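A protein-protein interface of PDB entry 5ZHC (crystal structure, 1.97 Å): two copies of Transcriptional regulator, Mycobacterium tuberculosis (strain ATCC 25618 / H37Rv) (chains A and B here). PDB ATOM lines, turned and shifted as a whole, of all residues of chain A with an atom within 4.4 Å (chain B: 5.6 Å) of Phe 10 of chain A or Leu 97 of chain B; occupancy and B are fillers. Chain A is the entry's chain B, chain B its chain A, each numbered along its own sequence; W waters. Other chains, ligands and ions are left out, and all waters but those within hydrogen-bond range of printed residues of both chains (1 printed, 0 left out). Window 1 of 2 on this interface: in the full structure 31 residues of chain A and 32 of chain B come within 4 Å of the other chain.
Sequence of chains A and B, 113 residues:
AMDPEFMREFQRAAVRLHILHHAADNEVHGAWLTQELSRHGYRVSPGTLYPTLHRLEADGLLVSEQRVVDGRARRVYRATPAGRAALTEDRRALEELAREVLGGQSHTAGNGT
OE1 of Glu 96 of chain B lies close to OE2 of Glu 100 of chain B, at 2.6 Å.
Among the printed residues, merely in contact across the chains: Phe 6 of chain A with Ala 13 of chain B, Met 7 of chain A with Ala 93 of chain B, Phe 10 of chain A with Ala 93 of chain B, Phe 10 of chain A with Leu 94 of chain B, Phe 10 of chain A with Leu 97 of chain B, Arg 12 of chain A with Glu 9 of chain B, Ala 13 of chain A with Glu 9 of chain B, Ala 14 of chain A with Leu 97 of chain B, His 18 of chain A with Leu 97 of chain B, His 18 of chain A with Val 101 of chain B, Tyr 42 of chain A with Glu 96 of chain B, Tyr 42 of chain A with Leu 97 of chain B, Leu 94 of chain A with Phe 10 of chain B, Leu 94 of chain A with Leu 94 of chain B, Leu 94 of chain A with Leu 97 of chain B, Leu 94 of chain A with Ala 98 of chain B and Leu 94 of chain A with Val 101 of chain B.
Water W1 bridges the side-chain hydroxyl of Tyr 42 of chain A (2.8 Å) and the backbone carbonyl oxygen of Ala 93 of chain B (2.9 Å).
Printed residues of chain B within 4 Å of Met 7 of chain A: Ala 93 (3.95 Å).
Printed residues of chain B within 4 Å of Ala 14 of chain A: Leu 97 (3.8 Å).
Printed residues of chain A within 4 Å of Ala 13 of chain B: Phe 6.
Of chain A, only Phe 10, Ala 14, His 18, Tyr 42 and Leu 94 come within 4 Å of Leu 97 of chain B.
Of the printed residues of chain A, Ala 98 of chain B touches Leu 94.
Of the printed residues of chain A, Val 101 of chain B touches His 18 and Leu 94.
The nearest residue of chain B that does not touch Phe 10 of chain A is Ala 13 of chain B (4.1 Å).
The nearest printed residue of chain A that does not touch Leu 97 of chain B is Ala 13 of chain A (5.1 Å).
Printed residues of chain A that touch a printed residue of chain B: Phe 6, Met 7, Phe 10, Arg 12, Ala 13, Ala 14, His 18, Tyr 42 and Leu 94.
Hydrophobic or aromatic side chains of chain A within 4 Å of the printed part of chain B: Phe 6, Met 7, Phe 10, Ala 14, His 18, Tyr 42 and Leu 94.
Of the 14 printed residues of chain B, 10 touch a printed residue of chain A.
Printed residues of chain B that touch a printed residue of chain A: Glu 9, Phe 10, Ala 13, Ala 93, Leu 94, Glu 96, Leu 97, Ala 98, Glu 100 and Val 101.
Among the printed residues, no Asp or Glu carboxylate lies within 4 Å of a Lys or Arg side-chain nitrogen of the other chain.
A ring nitrogen (NE2) of His 18 of chain A sits at hydrogen-bond distance from the side-chain carboxylate (OE1) of Glu 100 of chain B, at 2.7 Å.
The side-chain hydroxyl of Tyr 42 of chain A is in hydrogen-bond range of the side-chain carboxylate of Glu 100 of chain B (2.6 Å).
Phe 10 of chain A touches Leu 94 of chain B, and with the chains exchanged Leu 94 of chain A touches Phe 10 of chain B.
Ala 13 of chain A touches Glu 9 of chain B, but with the chains exchanged Glu 9 of chain A does not touch Ala 13 of chain B (4.2 Å).
Leu 94 of chain A touches its own counterpart, Leu 94 of chain B.
4 positions are printed for both chains.
Of the 19 pairs that touch across the chains among the printed residues, 3 have their exchanged pair printed and touching as well.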
ATOM      1  N   PHE A   6      -0.349  -4.277 -11.316  1.00  0.00           N
ATOM      2  CA  PHE A   6       1.036  -4.663 -11.020  1.00  0.00           C
ATOM      3  C   PHE A   6       1.985  -3.730 -11.783  1.00  0.00           C
ATOM      4  O   PHE A   6       2.926  -3.205 -11.203  1.00  0.00           O
ATOM      5  CB  PHE A   6       1.358  -6.093 -11.438  1.00  0.00           C
ATOM      6  CG  PHE A   6       2.834  -6.434 -11.286  1.00  0.00           C
ATOM      7  CD1 PHE A   6       3.353  -6.856 -10.073  1.00  0.00           C
ATOM      8  CD2 PHE A   6       3.714  -6.277 -12.347  1.00  0.00           C
ATOM      9  CE1 PHE A   6       4.699  -7.176  -9.936  1.00  0.00           C
ATOM     10  CE2 PHE A   6       5.073  -6.600 -12.223  1.00  0.00           C
ATOM     11  CZ  PHE A   6       5.562  -7.045 -11.018  1.00  0.00           C
ATOM     12  N   MET A   7       1.727  -3.534 -13.077  1.00  0.00           N
ATOM     13  CA  MET A   7       2.664  -2.785 -13.938  1.00  0.00           C
ATOM     14  C   MET A   7       2.800  -1.344 -13.486  1.00  0.00           C
ATOM     15  O   MET A   7       3.890  -0.785 -13.482  1.00  0.00           O
ATOM     16  CB  MET A   7       2.313  -2.896 -15.430  1.00  0.00           C
ATOM     17  CG  MET A   7       2.488  -4.297 -16.008  1.00  0.00           C
ATOM     18  SD  MET A   7       4.182  -4.933 -16.018  1.00  0.00           S
ATOM     19  CE  MET A   7       3.768  -6.512 -16.736  1.00  0.00           C
ATOM     20  N   ARG A   8       1.698  -0.747 -13.043  1.00  0.00           N
ATOM     21  CA  ARG A   8       1.751   0.614 -12.538  1.00  0.00           C
ATOM     22  C   ARG A   8       2.573   0.749 -11.268  1.00  0.00           C
ATOM     23  O   ARG A   8       3.455   1.609 -11.197  1.00  0.00           O
ATOM     24  CB  ARG A   8       0.347   1.154 -12.298  1.00  0.00           C
ATOM     25  CG  ARG A   8      -0.217   1.943 -13.444  1.00  0.00           C
ATOM     26  CD  ARG A   8      -1.378   2.789 -12.930  1.00  0.00           C
ATOM     27  NE  ARG A   8      -2.250   2.021 -12.026  1.00  0.00           N
ATOM     28  CZ  ARG A   8      -3.126   1.084 -12.407  1.00  0.00           C
ATOM     29  NH1 ARG A   8      -3.282   0.783 -13.697  1.00  0.00           N
ATOM     30  NH2 ARG A   8      -3.878   0.440 -11.493  1.00  0.00           N
ATOM     31  N   GLU A   9       2.301  -0.084 -10.272  1.00  0.00           N
ATOM     32  CA  GLU A   9       3.048  -0.045  -9.023  1.00  0.00           C
ATOM     33  C   GLU A   9       4.530  -0.374  -9.260  1.00  0.00           C
ATOM     34  O   GLU A   9       5.428   0.289  -8.740  1.00  0.00           O
ATOM     35  CB  GLU A   9       2.484  -1.088  -8.023  1.00  0.00           C
ATOM     36  N   PHE A  10       4.775  -1.406 -10.048  1.00  0.00           N
ATOM     37  CA  PHE A  10       6.137  -1.878 -10.294  1.00  0.00           C
ATOM     38  C   PHE A  10       6.911  -0.813 -11.045  1.00  0.00           C
ATOM     39  O   PHE A  10       8.050  -0.529 -10.721  1.00  0.00           O
ATOM     40  CB  PHE A  10       6.126  -3.167 -11.075  1.00  0.00           C
ATOM     41  CG  PHE A  10       7.476  -3.821 -11.156  1.00  0.00           C
ATOM     42  CD1 PHE A  10       8.001  -4.468 -10.061  1.00  0.00           C
ATOM     43  CD2 PHE A  10       8.226  -3.753 -12.320  1.00  0.00           C
ATOM     44  CE1 PHE A  10       9.237  -5.078 -10.117  1.00  0.00           C
ATOM     45  CE2 PHE A  10       9.479  -4.359 -12.393  1.00  0.00           C
ATOM     46  CZ  PHE A  10       9.966  -5.025 -11.309  1.00  0.00           C
ATOM     47  N   GLN A  11       6.289  -0.203 -12.040  1.00  0.00           N
ATOM     48  CA  GLN A  11       6.941   0.883 -12.783  1.00  0.00           C
ATOM     49  C   GLN A  11       7.327   2.090 -11.903  1.00  0.00           C
ATOM     50  O   GLN A  11       8.391   2.666 -12.099  1.00  0.00           O
ATOM     51  CB  GLN A  11       6.128   1.355 -13.976  1.00  0.00           C
ATOM     52  CG  GLN A  11       6.733   2.650 -14.528  1.00  0.00           C
ATOM     53  CD  GLN A  11       6.364   3.011 -15.942  1.00  0.00           C
ATOM     54  OE1 GLN A  11       6.112   4.198 -16.230  1.00  0.00           O
ATOM     55  NE2 GLN A  11       6.414   2.055 -16.837  1.00  0.00           N
ATOM     56  N   ARG A  12       6.483   2.482 -10.957  1.00  0.00           N
ATOM     57  CA  ARG A  12       6.827   3.560 -10.036  1.00  0.00           C
ATOM     58  C   ARG A  12       8.082   3.205  -9.254  1.00  0.00           C
ATOM     59  O   ARG A  12       8.996   4.027  -9.088  1.00  0.00           O
ATOM     60  CB  ARG A  12       5.703   3.861  -9.039  1.00  0.00           C
ATOM     61  CG  ARG A  12       4.460   4.453  -9.664  1.00  0.00           C
ATOM     62  CD  ARG A  12       3.398   4.810  -8.628  1.00  0.00           C
ATOM     63  NE  ARG A  12       2.077   4.871  -9.293  1.00  0.00           N
ATOM     64  CZ  ARG A  12       1.085   3.982  -9.169  1.00  0.00           C
ATOM     65  NH1 ARG A  12      -0.032   4.148  -9.869  1.00  0.00           N
ATOM     66  NH2 ARG A  12       1.166   2.936  -8.339  1.00  0.00           N
ATOM     67  N   ALA A  13       8.131   1.970  -8.779  1.00  0.00           N
ATOM     68  CA  ALA A  13       9.290   1.489  -8.054  1.00  0.00           C
ATOM     69  C   ALA A  13      10.520   1.449  -8.982  1.00  0.00           C
ATOM     70  O   ALA A  13      11.600   1.906  -8.616  1.00  0.00           O
ATOM     71  CB  ALA A  13       8.997   0.124  -7.455  1.00  0.00           C
ATOM     72  N   ALA A  14      10.351   0.894 -10.175  1.00  0.00           N
ATOM     73  CA  ALA A  14      11.445   0.797 -11.142  1.00  0.00           C
ATOM     74  C   ALA A  14      12.047   2.155 -11.498  1.00  0.00           C
ATOM     75  O   ALA A  14      13.261   2.314 -11.545  1.00  0.00           O
ATOM     76  CB  ALA A  14      10.996   0.073 -12.390  1.00  0.00           C
ATOM     77  N   HIS A  18      15.813   3.331 -10.920  1.00  0.00           N
ATOM     78  CA  HIS A  18      16.648   3.772 -12.040  1.00  0.00           C
ATOM     79  C   HIS A  18      17.240   5.153 -11.838  1.00  0.00           C
ATOM     80  O   HIS A  18      18.361   5.388 -12.198  1.00  0.00           O
ATOM     81  CB  HIS A  18      15.875   3.767 -13.393  1.00  0.00           C
ATOM     82  CG  HIS A  18      15.999   2.487 -14.143  1.00  0.00           C
ATOM     83  ND1 HIS A  18      17.003   2.270 -15.066  1.00  0.00           N
ATOM     84  CD2 HIS A  18      15.241   1.371 -14.139  1.00  0.00           C
ATOM     85  CE1 HIS A  18      16.867   1.058 -15.574  1.00  0.00           C
ATOM     86  NE2 HIS A  18      15.805   0.484 -15.027  1.00  0.00           N
ATOM     87  N   TYR A  42      10.603   2.359 -20.197  1.00  0.00           N
ATOM     88  CA  TYR A  42       9.690   2.972 -19.227  1.00  0.00           C
ATOM     89  C   TYR A  42       8.991   4.189 -19.832  1.00  0.00           C
ATOM     90  O   TYR A  42       9.615   5.030 -20.438  1.00  0.00           O
ATOM     91  CB  TYR A  42      10.413   3.314 -17.911  1.00  0.00           C
ATOM     92  CG  TYR A  42      11.004   2.053 -17.268  1.00  0.00           C
ATOM     93  CD1 TYR A  42      10.176   1.131 -16.621  1.00  0.00           C
ATOM     94  CD2 TYR A  42      12.356   1.735 -17.392  1.00  0.00           C
ATOM     95  CE1 TYR A  42      10.676  -0.041 -16.067  1.00  0.00           C
ATOM     96  CE2 TYR A  42      12.879   0.568 -16.857  1.00  0.00           C
ATOM     97  CZ  TYR A  42      12.031  -0.323 -16.191  1.00  0.00           C
ATOM     98  OH  TYR A  42      12.513  -1.488 -15.672  1.00  0.00           O
ATOM     99  N   LEU A  94      15.004  -5.926  -4.400  1.00  0.00           N
ATOM    100  CA  LEU A  94      14.784  -6.432  -5.773  1.00  0.00           C
ATOM    101  C   LEU A  94      15.442  -7.806  -5.966  1.00  0.00           C
ATOM    102  O   LEU A  94      14.812  -8.743  -6.437  1.00  0.00           O
ATOM    103  CB  LEU A  94      15.329  -5.443  -6.794  1.00  0.00           C
ATOM    104  CG  LEU A  94      15.273  -5.857  -8.279  1.00  0.00           C
ATOM    105  CD1 LEU A  94      13.827  -5.966  -8.668  1.00  0.00           C
ATOM    106  CD2 LEU A  94      16.083  -4.932  -9.156  1.00  0.00           C
ATOM    107  N   GLU B   9       5.804   1.031  -2.580  1.00  0.00           N
ATOM    108  CA  GLU B   9       5.411   0.702  -3.949  1.00  0.00           C
ATOM    109  C   GLU B   9       5.858  -0.710  -4.333  1.00  0.00           C
ATOM    110  O   GLU B   9       5.087  -1.494  -4.877  1.00  0.00           O
ATOM    111  CB  GLU B   9       6.020   1.707  -4.953  1.00  0.00           C
ATOM    112  CG  GLU B   9       5.554   3.164  -4.857  1.00  0.00           C
ATOM    113  CD  GLU B   9       6.527   4.210  -5.500  1.00  0.00           C
ATOM    114  OE1 GLU B   9       6.051   5.337  -5.814  1.00  0.00           O
ATOM    115  OE2 GLU B   9       7.765   3.954  -5.676  1.00  0.00           O
ATOM    116  N   PHE B  10       7.108  -1.030  -4.025  1.00  0.00           N
ATOM    117  CA  PHE B  10       7.706  -2.317  -4.410  1.00  0.00           C
ATOM    118  C   PHE B  10       6.969  -3.426  -3.677  1.00  0.00           C
ATOM    119  O   PHE B  10       6.632  -4.443  -4.281  1.00  0.00           O
ATOM    120  CB  PHE B  10       9.180  -2.352  -4.068  1.00  0.00           C
ATOM    121  CG  PHE B  10       9.898  -3.588  -4.542  1.00  0.00           C
ATOM    122  CD1 PHE B  10      10.218  -3.744  -5.871  1.00  0.00           C
ATOM    123  CD2 PHE B  10      10.205  -4.612  -3.653  1.00  0.00           C
ATOM    124  CE1 PHE B  10      10.853  -4.912  -6.318  1.00  0.00           C
ATOM    125  CE2 PHE B  10      10.843  -5.770  -4.086  1.00  0.00           C
ATOM    126  CZ  PHE B  10      11.169  -5.917  -5.414  1.00  0.00           C
ATOM    127  N   ALA B  13       3.602  -4.283  -5.211  1.00  0.00           N
ATOM    128  CA  ALA B  13       3.824  -5.061  -6.412  1.00  0.00           C
ATOM    129  C   ALA B  13       4.240  -6.513  -6.047  1.00  0.00           C
ATOM    130  O   ALA B  13       3.719  -7.466  -6.622  1.00  0.00           O
ATOM    131  CB  ALA B  13       4.886  -4.405  -7.273  1.00  0.00           C
ATOM    132  N   ARG B  92       8.372 -11.300 -16.049  1.00  0.00           N
ATOM    133  CA  ARG B  92       9.232 -10.704 -17.057  1.00  0.00           C
ATOM    134  C   ARG B  92       9.680  -9.291 -16.704  1.00  0.00           C
ATOM    135  O   ARG B  92      10.847  -8.914 -16.888  1.00  0.00           O
ATOM    136  CB  ARG B  92       8.580 -10.748 -18.434  1.00  0.00           C
ATOM    137  CG  ARG B  92       8.606 -12.148 -19.036  1.00  0.00           C
ATOM    138  N   ALA B  93       8.743  -8.506 -16.190  1.00  0.00           N
ATOM    139  CA  ALA B  93       9.027  -7.161 -15.754  1.00  0.00           C
ATOM    140  C   ALA B  93      10.082  -7.192 -14.629  1.00  0.00           C
ATOM    141  O   ALA B  93      11.049  -6.394 -14.629  1.00  0.00           O
ATOM    142  CB  ALA B  93       7.754  -6.464 -15.300  1.00  0.00           C
ATOM    143  N   LEU B  94       9.910  -8.114 -13.692  1.00  0.00           N
ATOM    144  CA  LEU B  94      10.870  -8.278 -12.601  1.00  0.00           C
ATOM    145  C   LEU B  94      12.268  -8.640 -13.141  1.00  0.00           C
ATOM    146  O   LEU B  94      13.278  -8.016 -12.769  1.00  0.00           O
ATOM    147  CB  LEU B  94      10.363  -9.339 -11.621  1.00  0.00           C
ATOM    148  CG  LEU B  94      11.267  -9.759 -10.468  1.00  0.00           C
ATOM    149  CD1 LEU B  94      11.606  -8.608  -9.582  1.00  0.00           C
ATOM    150  CD2 LEU B  94      10.520 -10.817  -9.657  1.00  0.00           C
ATOM    151  N   GLU B  95      12.311  -9.619 -14.029  1.00  0.00           N
ATOM    152  CA  GLU B  95      13.559 -10.045 -14.649  1.00  0.00           C
ATOM    153  C   GLU B  95      14.273  -8.865 -15.309  1.00  0.00           C
ATOM    154  O   GLU B  95      15.478  -8.690 -15.131  1.00  0.00           O
ATOM    155  CB  GLU B  95      13.329 -11.146 -15.692  1.00  0.00           C
ATOM    156  CG  GLU B  95      12.942 -12.496 -15.133  1.00  0.00           C
ATOM    157  CD  GLU B  95      12.388 -13.478 -16.179  1.00  0.00           C
ATOM    158  OE1 GLU B  95      12.171 -13.131 -17.386  1.00  0.00           O
ATOM    159  OE2 GLU B  95      12.167 -14.635 -15.794  1.00  0.00           O
ATOM    160  N   GLU B  96      13.524  -8.056 -16.051  1.00  0.00           N
ATOM    161  CA  GLU B  96      14.096  -6.933 -16.749  1.00  0.00           C
ATOM    162  C   GLU B  96      14.742  -5.916 -15.776  1.00  0.00           C
ATOM    163  O   GLU B  96      15.867  -5.420 -16.029  1.00  0.00           O
ATOM    164  CB  GLU B  96      13.080  -6.244 -17.676  1.00  0.00           C
ATOM    165  CG  GLU B  96      13.708  -5.008 -18.352  1.00  0.00           C
ATOM    166  CD  GLU B  96      12.781  -4.191 -19.235  1.00  0.00           C
ATOM    167  OE1 GLU B  96      12.792  -2.888 -19.230  1.00  0.00           O
ATOM    168  OE2 GLU B  96      12.047  -4.874 -19.962  1.00  0.00           O
ATOM    169  N   LEU B  97      14.044  -5.595 -14.696  1.00  0.00           N
ATOM    170  CA  LEU B  97      14.569  -4.619 -13.759  1.00  0.00           C
ATOM    171  C   LEU B  97      15.832  -5.149 -13.107  1.00  0.00           C
ATOM    172  O   LEU B  97      16.803  -4.417 -12.988  1.00  0.00           O
ATOM    173  CB  LEU B  97      13.531  -4.192 -12.721  1.00  0.00           C
ATOM    174  CG  LEU B  97      13.962  -3.098 -11.750  1.00  0.00           C
ATOM    175  CD1 LEU B  97      14.470  -1.829 -12.448  1.00  0.00           C
ATOM    176  CD2 LEU B  97      12.821  -2.787 -10.788  1.00  0.00           C
ATOM    177  N   ALA B  98      15.804  -6.409 -12.707  1.00  0.00           N
ATOM    178  CA  ALA B  98      16.986  -7.092 -12.190  1.00  0.00           C
ATOM    179  C   ALA B  98      18.181  -6.975 -13.149  1.00  0.00           C
ATOM    180  O   ALA B  98      19.256  -6.578 -12.700  1.00  0.00           O
ATOM    181  CB  ALA B  98      16.688  -8.546 -11.872  1.00  0.00           C
ATOM    182  N   ARG B  99      17.978  -7.218 -14.447  1.00  0.00           N
ATOM    183  CA  ARG B  99      19.068  -7.039 -15.450  1.00  0.00           C
ATOM    184  C   ARG B  99      19.607  -5.652 -15.560  1.00  0.00           C
ATOM    185  O   ARG B  99      20.797  -5.477 -15.709  1.00  0.00           O
ATOM    186  CB  ARG B  99      18.673  -7.480 -16.865  1.00  0.00           C
ATOM    187  CG  ARG B  99      18.450  -8.993 -16.921  1.00  0.00           C
ATOM    188  CD  ARG B  99      18.362  -9.490 -18.332  1.00  0.00           C
ATOM    189  NE  ARG B  99      17.342  -8.818 -19.127  1.00  0.00           N
ATOM    190  CZ  ARG B  99      16.064  -9.162 -19.263  1.00  0.00           C
ATOM    191  NH1 ARG B  99      15.546 -10.234 -18.644  1.00  0.00           N
ATOM    192  NH2 ARG B  99      15.290  -8.451 -20.069  1.00  0.00           N
ATOM    193  N   GLU B 100      18.713  -4.678 -15.471  1.00  0.00           N
ATOM    194  CA  GLU B 100      19.046  -3.275 -15.630  1.00  0.00           C
ATOM    195  C   GLU B 100      19.878  -2.701 -14.491  1.00  0.00           C
ATOM    196  O   GLU B 100      20.871  -2.022 -14.730  1.00  0.00           O
ATOM    197  CB  GLU B 100      17.739  -2.467 -15.762  1.00  0.00           C
ATOM    198  CG  GLU B 100      17.113  -2.637 -17.154  1.00  0.00           C
ATOM    199  CD  GLU B 100      15.658  -2.213 -17.210  1.00  0.00           C
ATOM    200  OE1 GLU B 100      15.071  -1.884 -16.158  1.00  0.00           O
ATOM    201  OE2 GLU B 100      15.107  -2.236 -18.328  1.00  0.00           O
ATOM    202  N   VAL B 101      19.478  -2.977 -13.248  1.00  0.00           N
ATOM    203  CA  VAL B 101      20.068  -2.258 -12.107  1.00  0.00           C
ATOM    204  C   VAL B 101      20.996  -3.101 -11.210  1.00  0.00           C
ATOM    205  O   VAL B 101      21.642  -2.534 -10.326  1.00  0.00           O
ATOM    206  CB  VAL B 101      19.003  -1.491 -11.268  1.00  0.00           C
ATOM    207  CG1 VAL B 101      18.269  -0.454 -12.124  1.00  0.00           C
ATOM    208  CG2 VAL B 101      18.056  -2.426 -10.531  1.00  0.00           C
ATOM    209  N   LEU B 102      21.091  -4.414 -11.446  1.00  0.00           N
ATOM    210  CA  LEU B 102      22.004  -5.294 -10.695  1.00  0.00           C
ATOM    211  C   LEU B 102      23.125  -5.770 -11.617  1.00  0.00           C
ATOM    212  O   LEU B 102      24.098  -6.357 -11.234  1.00  0.00           O
ATOM    213  CB  LEU B 102      21.266  -6.509 -10.134  1.00  0.00           C
ATOM    214  CG  LEU B 102      19.971  -6.255  -9.341  1.00  0.00           C
ATOM    215  CD1 LEU B 102      19.275  -7.553  -9.018  1.00  0.00           C
ATOM    216  CD2 LEU B 102      20.261  -5.504  -8.053  1.00  0.00           C
HETATM  217  O   HOH W   1      10.806  -3.755 -15.803  1.00  0.00           O
